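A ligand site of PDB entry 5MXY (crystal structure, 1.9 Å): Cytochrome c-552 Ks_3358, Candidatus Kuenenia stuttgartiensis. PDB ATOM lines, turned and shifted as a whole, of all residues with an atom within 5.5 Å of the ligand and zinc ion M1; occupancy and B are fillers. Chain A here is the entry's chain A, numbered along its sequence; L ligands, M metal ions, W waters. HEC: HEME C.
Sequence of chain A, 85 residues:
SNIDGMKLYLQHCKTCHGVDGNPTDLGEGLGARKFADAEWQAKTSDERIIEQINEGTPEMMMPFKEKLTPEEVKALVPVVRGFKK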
ATOM      1  N   TYR A   9      13.363  12.441  29.249  1.00  0.00           N
ATOM      2  CA  TYR A   9      14.202  13.034  28.201  1.00  0.00           C
ATOM      3  C   TYR A   9      14.530  14.502  28.496  1.00  0.00           C
ATOM      4  O   TYR A   9      15.683  14.921  28.361  1.00  0.00           O
ATOM      5  CB  TYR A   9      13.540  12.887  26.820  1.00  0.00           C
ATOM      6  CG  TYR A   9      14.355  13.471  25.686  1.00  0.00           C
ATOM      7  CD1 TYR A   9      14.213  14.814  25.323  1.00  0.00           C
ATOM      8  CD2 TYR A   9      15.261  12.676  24.967  1.00  0.00           C
ATOM      9  CE1 TYR A   9      14.956  15.364  24.291  1.00  0.00           C
ATOM     10  CE2 TYR A   9      16.012  13.221  23.920  1.00  0.00           C
ATOM     11  CZ  TYR A   9      15.857  14.561  23.592  1.00  0.00           C
ATOM     12  OH  TYR A   9      16.592  15.117  22.560  1.00  0.00           O
ATOM     13  N   HIS A  12      16.998  14.609  31.496  1.00  0.00           N
ATOM     14  CA  HIS A  12      18.305  13.932  31.412  1.00  0.00           C
ATOM     15  C   HIS A  12      19.047  14.026  30.084  1.00  0.00           C
ATOM     16  O   HIS A  12      20.251  13.802  30.037  1.00  0.00           O
ATOM     17  CB  HIS A  12      18.167  12.454  31.793  1.00  0.00           C
ATOM     18  CG  HIS A  12      17.727  12.223  33.213  1.00  0.00           C
ATOM     19  ND1 HIS A  12      18.511  12.547  34.292  1.00  0.00           N
ATOM     20  CD2 HIS A  12      16.592  11.673  33.713  1.00  0.00           C
ATOM     21  CE1 HIS A  12      17.872  12.223  35.409  1.00  0.00           C
ATOM     22  NE2 HIS A  12      16.712  11.694  35.080  1.00  0.00           N
ATOM     23  N   CYS A  13      18.333  14.348  29.006  1.00  0.00           N
ATOM     24  CA  CYS A  13      18.894  14.208  27.655  1.00  0.00           C
ATOM     25  C   CYS A  13      18.914  15.496  26.844  1.00  0.00           C
ATOM     26  O   CYS A  13      19.813  15.679  26.017  1.00  0.00           O
ATOM     27  CB  CYS A  13      18.137  13.132  26.868  1.00  0.00           C
ATOM     28  SG  CYS A  13      17.704  11.647  27.826  1.00  0.00           S
ATOM     29  N   THR A  15      19.668  18.578  27.378  1.00  0.00           N
ATOM     30  CA  THR A  15      20.834  19.470  27.532  1.00  0.00           C
ATOM     31  C   THR A  15      21.925  19.211  26.479  1.00  0.00           C
ATOM     32  O   THR A  15      22.694  20.111  26.152  1.00  0.00           O
ATOM     33  CB  THR A  15      21.462  19.425  28.938  1.00  0.00           C
ATOM     34  OG1 THR A  15      21.743  18.064  29.302  1.00  0.00           O
ATOM     35  CG2 THR A  15      20.536  20.061  29.970  1.00  0.00           C
ATOM     36  N   CYS A  16      21.974  17.984  25.963  1.00  0.00           N
ATOM     37  CA  CYS A  16      22.890  17.649  24.872  1.00  0.00           C
ATOM     38  C   CYS A  16      22.172  17.426  23.534  1.00  0.00           C
ATOM     39  O   CYS A  16      22.637  17.895  22.496  1.00  0.00           O
ATOM     40  CB  CYS A  16      23.733  16.429  25.201  1.00  0.00           C
ATOM     41  SG  CYS A  16      25.030  16.670  26.445  1.00  0.00           S
ATOM     42  N   HIS A  17      21.039  16.712  23.572  1.00  0.00           N
ATOM     43  CA  HIS A  17      20.332  16.334  22.342  1.00  0.00           C
ATOM     44  C   HIS A  17      19.272  17.317  21.853  1.00  0.00           C
ATOM     45  O   HIS A  17      18.788  17.186  20.733  1.00  0.00           O
ATOM     46  CB  HIS A  17      19.780  14.911  22.444  1.00  0.00           C
ATOM     47  CG  HIS A  17      20.844  13.864  22.472  1.00  0.00           C
ATOM     48  ND1 HIS A  17      21.567  13.511  21.355  1.00  0.00           N
ATOM     49  CD2 HIS A  17      21.314  13.100  23.487  1.00  0.00           C
ATOM     50  CE1 HIS A  17      22.440  12.574  21.681  1.00  0.00           C
ATOM     51  NE2 HIS A  17      22.303  12.301  22.961  1.00  0.00           N
ATOM     52  N   LEU A  26      26.568  22.310  23.429  1.00  0.00           N
ATOM     53  CA  LEU A  26      27.262  21.293  24.235  1.00  0.00           C
ATOM     54  C   LEU A  26      27.304  19.919  23.542  1.00  0.00           C
ATOM     55  O   LEU A  26      28.370  19.327  23.404  1.00  0.00           O
ATOM     56  CB  LEU A  26      26.640  21.171  25.633  1.00  0.00           C
ATOM     57  CG  LEU A  26      27.184  20.127  26.618  1.00  0.00           C
ATOM     58  CD1 LEU A  26      28.647  20.344  26.982  1.00  0.00           C
ATOM     59  CD2 LEU A  26      26.334  20.078  27.883  1.00  0.00           C
ATOM     60  N   GLY A  27      26.135  19.432  23.125  1.00  0.00           N
ATOM     61  CA  GLY A  27      25.999  18.120  22.477  1.00  0.00           C
ATOM     62  C   GLY A  27      26.796  17.987  21.188  1.00  0.00           C
ATOM     63  O   GLY A  27      27.514  16.997  21.003  1.00  0.00           O
ATOM     64  N   LEU A  30      30.535  17.783  21.714  1.00  0.00           N
ATOM     65  CA  LEU A  30      30.872  16.452  22.237  1.00  0.00           C
ATOM     66  C   LEU A  30      30.791  15.333  21.196  1.00  0.00           C
ATOM     67  O   LEU A  30      31.402  14.265  21.370  1.00  0.00           O
ATOM     68  CB  LEU A  30      29.989  16.120  23.442  1.00  0.00           C
ATOM     69  CG  LEU A  30      30.292  16.887  24.734  1.00  0.00           C
ATOM     70  CD1 LEU A  30      29.086  16.808  25.664  1.00  0.00           C
ATOM     71  CD2 LEU A  30      31.547  16.390  25.417  1.00  0.00           C
ATOM     72  N   GLY A  31      30.019  15.564  20.130  1.00  0.00           N
ATOM     73  CA  GLY A  31      29.969  14.638  18.999  1.00  0.00           C
ATOM     74  C   GLY A  31      28.600  14.155  18.570  1.00  0.00           C
ATOM     75  O   GLY A  31      28.513  13.297  17.679  1.00  0.00           O
ATOM     76  N   ALA A  32      27.541  14.695  19.173  1.00  0.00           N
ATOM     77  CA  ALA A  32      26.169  14.265  18.884  1.00  0.00           C
ATOM     78  C   ALA A  32      25.676  14.775  17.534  1.00  0.00           C
ATOM     79  O   ALA A  32      26.010  15.887  17.111  1.00  0.00           O
ATOM     80  CB  ALA A  32      25.216  14.697  19.997  1.00  0.00           C
ATOM     81  N   ARG A  33      24.887  13.928  16.865  1.00  0.00           N
ATOM     82  CA  ARG A  33      24.233  14.259  15.590  1.00  0.00           C
ATOM     83  C   ARG A  33      22.721  14.335  15.811  1.00  0.00           C
ATOM     84  O   ARG A  33      22.234  13.917  16.866  1.00  0.00           O
ATOM     85  CB  ARG A  33      24.565  13.217  14.520  1.00  0.00           C
ATOM     86  CG  ARG A  33      25.974  13.291  13.955  1.00  0.00           C
ATOM     87  CD  ARG A  33      26.922  12.344  14.693  1.00  0.00           C
ATOM     88  NE  ARG A  33      28.187  12.158  13.983  1.00  0.00           N
ATOM     89  CZ  ARG A  33      28.547  11.064  13.314  1.00  0.00           C
ATOM     90  NH1 ARG A  33      27.736  10.022  13.231  1.00  0.00           N
ATOM     91  NH2 ARG A  33      29.730  11.009  12.734  1.00  0.00           N
ATOM     92  N   PHE A  35      18.736  13.572  15.737  1.00  0.00           N
ATOM     93  CA  PHE A  35      17.849  12.410  15.749  1.00  0.00           C
ATOM     94  C   PHE A  35      16.848  12.415  14.588  1.00  0.00           C
ATOM     95  O   PHE A  35      16.537  11.346  14.036  1.00  0.00           O
ATOM     96  CB  PHE A  35      17.101  12.291  17.095  1.00  0.00           C
ATOM     97  CG  PHE A  35      17.963  11.828  18.249  1.00  0.00           C
ATOM     98  CD1 PHE A  35      18.959  10.854  18.070  1.00  0.00           C
ATOM     99  CD2 PHE A  35      17.759  12.335  19.531  1.00  0.00           C
ATOM    100  CE1 PHE A  35      19.742  10.425  19.140  1.00  0.00           C
ATOM    101  CE2 PHE A  35      18.538  11.917  20.609  1.00  0.00           C
ATOM    102  CZ  PHE A  35      19.531  10.957  20.410  1.00  0.00           C
ATOM    103  N   TRP A  40      19.608   7.933   9.682  1.00  0.00           N
ATOM    104  CA  TRP A  40      20.027   7.492  11.014  1.00  0.00           C
ATOM    105  C   TRP A  40      18.974   6.567  11.647  1.00  0.00           C
ATOM    106  O   TRP A  40      19.311   5.485  12.114  1.00  0.00           O
ATOM    107  CB  TRP A  40      20.369   8.659  11.958  1.00  0.00           C
ATOM    108  CG  TRP A  40      20.788   8.151  13.321  1.00  0.00           C
ATOM    109  CD1 TRP A  40      22.033   7.694  13.680  1.00  0.00           C
ATOM    110  CD2 TRP A  40      19.956   8.001  14.471  1.00  0.00           C
ATOM    111  NE1 TRP A  40      22.028   7.279  14.993  1.00  0.00           N
ATOM    112  CE2 TRP A  40      20.775   7.458  15.504  1.00  0.00           C
ATOM    113  CE3 TRP A  40      18.603   8.264  14.746  1.00  0.00           C
ATOM    114  CZ2 TRP A  40      20.274   7.189  16.785  1.00  0.00           C
ATOM    115  CZ3 TRP A  40      18.107   8.001  16.020  1.00  0.00           C
ATOM    116  CH2 TRP A  40      18.951   7.459  17.025  1.00  0.00           C
ATOM    117  N   THR A  44      19.462   2.394  12.625  1.00  0.00           N
ATOM    118  CA  THR A  44      19.578   2.257  14.084  1.00  0.00           C
ATOM    119  C   THR A  44      18.455   1.376  14.648  1.00  0.00           C
ATOM    120  O   THR A  44      17.273   1.661  14.431  1.00  0.00           O
ATOM    121  CB  THR A  44      19.598   3.629  14.770  1.00  0.00           C
ATOM    122  OG1 THR A  44      20.675   4.418  14.226  1.00  0.00           O
ATOM    123  CG2 THR A  44      19.788   3.518  16.290  1.00  0.00           C
ATOM    124  N   ARG A  48      20.248  -0.870  19.897  1.00  0.00           N
ATOM    125  CA  ARG A  48      21.364   0.071  19.785  1.00  0.00           C
ATOM    126  C   ARG A  48      21.083   1.341  20.599  1.00  0.00           C
ATOM    127  O   ARG A  48      21.993   1.871  21.250  1.00  0.00           O
ATOM    128  CB  ARG A  48      21.661   0.400  18.314  1.00  0.00           C
ATOM    129  CG  ARG A  48      22.613   1.566  18.026  1.00  0.00           C
ATOM    130  CD  ARG A  48      24.095   1.188  18.085  1.00  0.00           C
ATOM    131  NE  ARG A  48      24.597   0.966  19.452  1.00  0.00           N
ATOM    132  CZ  ARG A  48      25.045   1.920  20.266  1.00  0.00           C
ATOM    133  NH1 ARG A  48      25.076   3.192  19.893  1.00  0.00           N
ATOM    134  NH2 ARG A  48      25.471   1.593  21.480  1.00  0.00           N
ATOM    135  N   ILE A  49      19.834   1.824  20.554  1.00  0.00           N
ATOM    136  CA  ILE A  49      19.406   2.987  21.334  1.00  0.00           C
ATOM    137  C   ILE A  49      19.476   2.657  22.826  1.00  0.00           C
ATOM    138  O   ILE A  49      19.984   3.478  23.602  1.00  0.00           O
ATOM    139  CB  ILE A  49      17.980   3.493  20.912  1.00  0.00           C
ATOM    140  CG1 ILE A  49      18.023   4.095  19.495  1.00  0.00           C
ATOM    141  CG2 ILE A  49      17.428   4.516  21.905  1.00  0.00           C
ATOM    142  CD1 ILE A  49      16.681   4.187  18.783  1.00  0.00           C
ATOM    143  N   GLN A  52      23.210   2.345  23.925  1.00  0.00           N
ATOM    144  CA  GLN A  52      23.777   3.691  24.036  1.00  0.00           C
ATOM    145  C   GLN A  52      23.358   4.410  25.326  1.00  0.00           C
ATOM    146  O   GLN A  52      24.211   4.962  26.020  1.00  0.00           O
ATOM    147  CB  GLN A  52      23.436   4.538  22.804  1.00  0.00           C
ATOM    148  CG  GLN A  52      24.139   5.888  22.798  1.00  0.00           C
ATOM    149  CD  GLN A  52      25.637   5.792  22.611  1.00  0.00           C
ATOM    150  OE1 GLN A  52      26.123   4.910  21.891  1.00  0.00           O
ATOM    151  NE2 GLN A  52      26.387   6.670  23.268  1.00  0.00           N
ATOM    152  N   ILE A  53      22.066   4.405  25.636  1.00  0.00           N
ATOM    153  CA  ILE A  53      21.571   4.979  26.890  1.00  0.00           C
ATOM    154  C   ILE A  53      22.239   4.311  28.101  1.00  0.00           C
ATOM    155  O   ILE A  53      22.732   5.007  28.993  1.00  0.00           O
ATOM    156  CB  ILE A  53      20.031   4.944  27.015  1.00  0.00           C
ATOM    157  CG1 ILE A  53      19.371   5.717  25.863  1.00  0.00           C
ATOM    158  CG2 ILE A  53      19.582   5.555  28.351  1.00  0.00           C
ATOM    159  CD1 ILE A  53      17.924   5.351  25.599  1.00  0.00           C
ATOM    160  N   THR A  57      29.196   6.551  25.686  1.00  0.00           N
ATOM    161  CA  THR A  57      30.396   6.518  24.860  1.00  0.00           C
ATOM    162  C   THR A  57      31.459   7.303  25.629  1.00  0.00           C
ATOM    163  O   THR A  57      31.201   8.431  26.062  1.00  0.00           O
ATOM    164  CB  THR A  57      30.155   7.175  23.486  1.00  0.00           C
ATOM    165  OG1 THR A  57      29.092   6.498  22.805  1.00  0.00           O
ATOM    166  CG2 THR A  57      31.407   7.115  22.609  1.00  0.00           C
ATOM    167  N   MET A  60      32.189  11.210  25.559  1.00  0.00           N
ATOM    168  CA  MET A  60      31.110  11.765  24.728  1.00  0.00           C
ATOM    169  C   MET A  60      29.765  11.813  25.453  1.00  0.00           C
ATOM    170  O   MET A  60      29.146  12.872  25.540  1.00  0.00           O
ATOM    171  CB  MET A  60      30.995  10.979  23.409  1.00  0.00           C
ATOM    172  CG  MET A  60      32.221  11.066  22.516  1.00  0.00           C
ATOM    173  SD  MET A  60      31.866  10.550  20.825  1.00  0.00           S
ATOM    174  CE  MET A  60      33.530  10.285  20.222  1.00  0.00           C
ATOM    175  N   MET A  61      29.334  10.667  25.979  1.00  0.00           N
ATOM    176  CA  MET A  61      28.044  10.545  26.640  1.00  0.00           C
ATOM    177  C   MET A  61      28.222   9.621  27.842  1.00  0.00           C
ATOM    178  O   MET A  61      28.791   8.533  27.723  1.00  0.00           O
ATOM    179  CB  MET A  61      27.010   9.973  25.664  1.00  0.00           C
ATOM    180  CG  MET A  61      25.605   9.807  26.221  1.00  0.00           C
ATOM    181  SD  MET A  61      24.379   9.248  25.000  1.00  0.00           S
ATOM    182  CE  MET A  61      23.425   8.209  26.100  1.00  0.00           C
ATOM    183  N   MET A  62      27.752  10.068  29.008  1.00  0.00           N
ATOM    184  CA  MET A  62      27.825   9.269  30.225  1.00  0.00           C
ATOM    185  C   MET A  62      26.916   8.035  30.138  1.00  0.00           C
ATOM    186  O   MET A  62      25.878   8.093  29.464  1.00  0.00           O
ATOM    187  CB  MET A  62      27.502  10.115  31.470  1.00  0.00           C
ATOM    188  CG  MET A  62      26.093  10.693  31.544  1.00  0.00           C
ATOM    189  SD  MET A  62      25.816  12.090  30.431  1.00  0.00           S
ATOM    190  CE  MET A  62      26.444  13.445  31.411  1.00  0.00           C
ATOM    191  N   PHE A  64      23.962   5.704  31.503  1.00  0.00           N
ATOM    192  CA  PHE A  64      22.769   5.975  32.328  1.00  0.00           C
ATOM    193  C   PHE A  64      22.233   4.760  33.101  1.00  0.00           C
ATOM    194  O   PHE A  64      21.231   4.876  33.803  1.00  0.00           O
ATOM    195  CB  PHE A  64      21.645   6.602  31.488  1.00  0.00           C
ATOM    196  CG  PHE A  64      21.850   8.061  31.213  1.00  0.00           C
ATOM    197  CD1 PHE A  64      22.600   8.479  30.091  1.00  0.00           C
ATOM    198  CD2 PHE A  64      21.306   9.038  32.060  1.00  0.00           C
ATOM    199  CE1 PHE A  64      22.792   9.837  29.849  1.00  0.00           C
ATOM    200  CE2 PHE A  64      21.494  10.392  31.811  1.00  0.00           C
ATOM    201  CZ  PHE A  64      22.243  10.791  30.702  1.00  0.00           C
ATOM    202  N   LEU A  68      19.030   5.095  35.549  1.00  0.00           N
ATOM    203  CA  LEU A  68      17.691   4.718  35.088  1.00  0.00           C
ATOM    204  C   LEU A  68      17.504   3.203  35.061  1.00  0.00           C
ATOM    205  O   LEU A  68      18.436   2.468  34.709  1.00  0.00           O
ATOM    206  CB  LEU A  68      17.413   5.265  33.675  1.00  0.00           C
ATOM    207  CG  LEU A  68      17.709   6.732  33.330  1.00  0.00           C
ATOM    208  CD1 LEU A  68      17.796   6.905  31.828  1.00  0.00           C
ATOM    209  CD2 LEU A  68      16.677   7.683  33.926  1.00  0.00           C
ATOM    210  N   LEU A  76      12.341   5.632  26.807  1.00  0.00           N
ATOM    211  CA  LEU A  76      13.004   6.669  26.014  1.00  0.00           C
ATOM    212  C   LEU A  76      13.072   6.344  24.518  1.00  0.00           C
ATOM    213  O   LEU A  76      13.263   7.247  23.704  1.00  0.00           O
ATOM    214  CB  LEU A  76      14.404   6.990  26.557  1.00  0.00           C
ATOM    215  CG  LEU A  76      14.468   7.723  27.898  1.00  0.00           C
ATOM    216  CD1 LEU A  76      15.773   7.435  28.614  1.00  0.00           C
ATOM    217  CD2 LEU A  76      14.273   9.216  27.704  1.00  0.00           C
ATOM    218  N   VAL A  80      13.058   9.149  21.209  1.00  0.00           N
ATOM    219  CA  VAL A  80      14.108   9.195  20.203  1.00  0.00           C
ATOM    220  C   VAL A  80      13.549   8.937  18.787  1.00  0.00           C
ATOM    221  O   VAL A  80      13.905   9.653  17.833  1.00  0.00           O
ATOM    222  CB  VAL A  80      15.264   8.198  20.543  1.00  0.00           C
ATOM    223  CG1 VAL A  80      16.247   8.068  19.400  1.00  0.00           C
ATOM    224  CG2 VAL A  80      15.998   8.642  21.808  1.00  0.00           C
HETATM  225 FE   HEC L   1      23.299  10.824  24.030  1.00  0.00          FE
HETATM  226  CHA HEC L   1      24.774   9.472  21.215  1.00  0.00           C
HETATM  227  CHB HEC L   1      20.447   9.025  23.426  1.00  0.00           C
HETATM  228  CHC HEC L   1      22.082  11.789  27.101  1.00  0.00           C
HETATM  229  CHD HEC L   1      25.795  13.184  24.243  1.00  0.00           C
HETATM  230  NA  HEC L   1      22.718   9.445  22.567  1.00  0.00           N
HETATM  231  C1A HEC L   1      23.391   9.059  21.460  1.00  0.00           C
HETATM  232  C2A HEC L   1      22.660   8.088  20.589  1.00  0.00           C
HETATM  233  C3A HEC L   1      21.366   7.960  21.258  1.00  0.00           C
HETATM  234  C4A HEC L   1      21.516   8.849  22.437  1.00  0.00           C
HETATM  235  CMA HEC L   1      20.181   7.127  20.824  1.00  0.00           C
HETATM  236  CAA HEC L   1      23.050   7.448  19.278  1.00  0.00           C
HETATM  237  CBA HEC L   1      23.952   6.244  19.262  1.00  0.00           C
HETATM  238  CGA HEC L   1      24.053   5.760  17.824  1.00  0.00           C
HETATM  239  O1A HEC L   1      24.095   6.578  16.873  1.00  0.00           O
HETATM  240  O2A HEC L   1      24.118   4.532  17.641  1.00  0.00           O
HETATM  241  NB  HEC L   1      21.562  10.442  25.109  1.00  0.00           N
HETATM  242  C1B HEC L   1      20.489   9.717  24.715  1.00  0.00           C
HETATM  243  C2B HEC L   1      19.372   9.636  25.688  1.00  0.00           C
HETATM  244  C3B HEC L   1      19.889  10.465  26.770  1.00  0.00           C
HETATM  245  C4B HEC L   1      21.208  10.922  26.308  1.00  0.00           C
HETATM  246  CMB HEC L   1      18.057   8.910  25.560  1.00  0.00           C
HETATM  247  CAB HEC L   1      19.247  10.781  28.063  1.00  0.00           C
HETATM  248  CBB HEC L   1      19.071   9.643  29.034  1.00  0.00           C
HETATM  249  NC  HEC L   1      23.858  12.241  25.468  1.00  0.00           N
HETATM  250  C1C HEC L   1      23.239  12.545  26.626  1.00  0.00           C
HETATM  251  C2C HEC L   1      23.849  13.644  27.427  1.00  0.00           C
HETATM  252  C3C HEC L   1      24.951  14.043  26.544  1.00  0.00           C
HETATM  253  C4C HEC L   1      24.865  13.138  25.379  1.00  0.00           C
HETATM  254  CMC HEC L   1      23.414  14.191  28.758  1.00  0.00           C
HETATM  255  CAC HEC L   1      25.941  15.126  26.790  1.00  0.00           C
HETATM  256  CBC HEC L   1      26.981  14.867  27.844  1.00  0.00           C
HETATM  257  ND  HEC L   1      25.030  11.232  22.925  1.00  0.00           N
HETATM  258  C1D HEC L   1      25.930  12.219  23.126  1.00  0.00           C
HETATM  259  C2D HEC L   1      27.061  12.253  22.163  1.00  0.00           C
HETATM  260  C3D HEC L   1      26.749  11.138  21.259  1.00  0.00           C
HETATM  261  C4D HEC L   1      25.487  10.600  21.822  1.00  0.00           C
HETATM  262  CMD HEC L   1      28.232  13.197  22.123  1.00  0.00           C
HETATM  263  CAD HEC L   1      27.528  10.633  20.066  1.00  0.00           C
HETATM  264  CBD HEC L   1      28.354   9.444  20.582  1.00  0.00           C
HETATM  265  CGD HEC L   1      28.071   8.127  19.860  1.00  0.00           C
HETATM  266  O1D HEC L   1      28.719   7.095  20.188  1.00  0.00           O
HETATM  267  O2D HEC L   1      27.207   8.081  18.960  1.00  0.00           O
HETATM  268 ZN    ZN M   1      29.153   5.214  19.253  1.00  0.00          ZN
HETATM  269 ZN    ZN M   2      27.297   2.497  23.565  1.00  0.00          ZN
HETATM  270  O   HOH W   1      27.614   5.548  17.927  1.00  0.00           O
HETATM  271  O   HOH W   2      28.237   4.062  20.827  1.00  0.00           O
HETATM  272  O   HOH W   3      26.283   4.176  16.031  1.00  0.00           O
HETATM  273  O   HOH W   4      23.406   3.886  15.088  1.00  0.00           O
HETATM  274  O   HOH W   5      25.452   9.084  17.119  1.00  0.00           O
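The side-chain sulfur (SD) of Met 61 is bound to an iron atom (FE) of the ligand (2.1 Å). The side-chain hydroxyl (OG1) of Thr 57 sits close to an oxygen (O1D) of the ligand (2.7 Å). SG of Cys 13 is bonded to CAB of the ligand (1.8 Å). An iron atom (FE) of the ligand is bound by a ring nitrogen (NE2) of His 17 (2.1 Å). NH1 of Arg 48 is in salt-bridge range of O2A of the ligand. The side-chain sulfur (SG) of Cys 16 is covalently linked to a carbon (CAC) of the ligand (1.8 Å). The indole nitrogen of Trp 40 is in hydrogen-bond range of an oxygen (O1A) of the ligand (2.9 Å).
The side-chain hydroxyl of Thr 57 lies within hydrogen-bond range of the side-chain amide nitrogen of Gln 52, at 2.7 Å. N of Ala 32 lies within hydrogen-bond range of O of Gly 27 (2.9 Å). The side-chain amide oxygen (OE1) of Gln 52 is in hydrogen-bond range of the guanidinium group (NH1) of Arg 48 (2.8 Å). The side-chain amide nitrogen (NE2) of Gln 52 sits close to the side-chain sulfur (SD) of Met 61 (3.7 Å). The side-chain hydroxyl (OG1) of Thr 44 sits at hydrogen-bond distance from the backbone carbonyl oxygen (O) of Trp 40 (2.7 Å). The backbone NH of Phe 64 lies within hydrogen-bond range of the backbone carbonyl oxygen of Ile 53 (2.9 Å).
His 12 touches the ligand (O to CMC, 3.4 Å). O of Leu 30 touches CMD of the ligand (3.4 Å). Gly 31 touches the ligand. Ala 32 touches the ligand. Phe 35 touches the ligand. Ile 49 touches the ligand (CG2 to CMA, 3.9 Å). Gln 52 touches the ligand. CG1 of Ile 53 touches CMB of the ligand (3.5 Å). Met 60 touches the ligand. SD of Met 62 touches CMC of the ligand (3.6 Å). CE1 of Phe 64 touches CHC of the ligand, 3.4 Å away. CD1 of Leu 76 touches CBB of the ligand, 3.99 Å away. Hydrophobic or aromatic side chains within 4 Å of the ligand: His 17, Leu 30, Ala 32, Phe 35, Trp 40, Ile 49, Ile 53, Met 60, Met 61, Met 62, Phe 64 and Leu 76. 19 residues have an atom within 4 Å of the ligand: His 12, Cys 13, Cys 16, His 17, Leu 30, Gly 31, Ala 32, Phe 35, Trp 40, Arg 48, Ile 49, Gln 52, Ile 53, Thr 57, Met 60, Met 61, Met 62, Phe 64 and Leu 76. The nearest printed residue that does not touch the ligand is Gly 27 (4.03 Å).
Thr 57 touches zinc ion M1. Of the 27 residues printed, 1 comes within 4 Å of zinc ion M1.
Zinc ion M1 is bound by water W1 (2.1 Å), O1D of the ligand (2.1 Å) and water W2 (2.2 Å).
Water W2 lies within hydrogen-bond range of the side-chain amide oxygen (OE1) of Gln 52 (2.5 Å), the side-chain hydroxyl (OG1) of Thr 57 (3.3 Å) and the guanidinium group (NH1) of Arg 48 (3.4 Å). Water W4 bridges an oxygen (O2A) of the ligand and the side-chain hydroxyl (OG1) of Thr 44.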
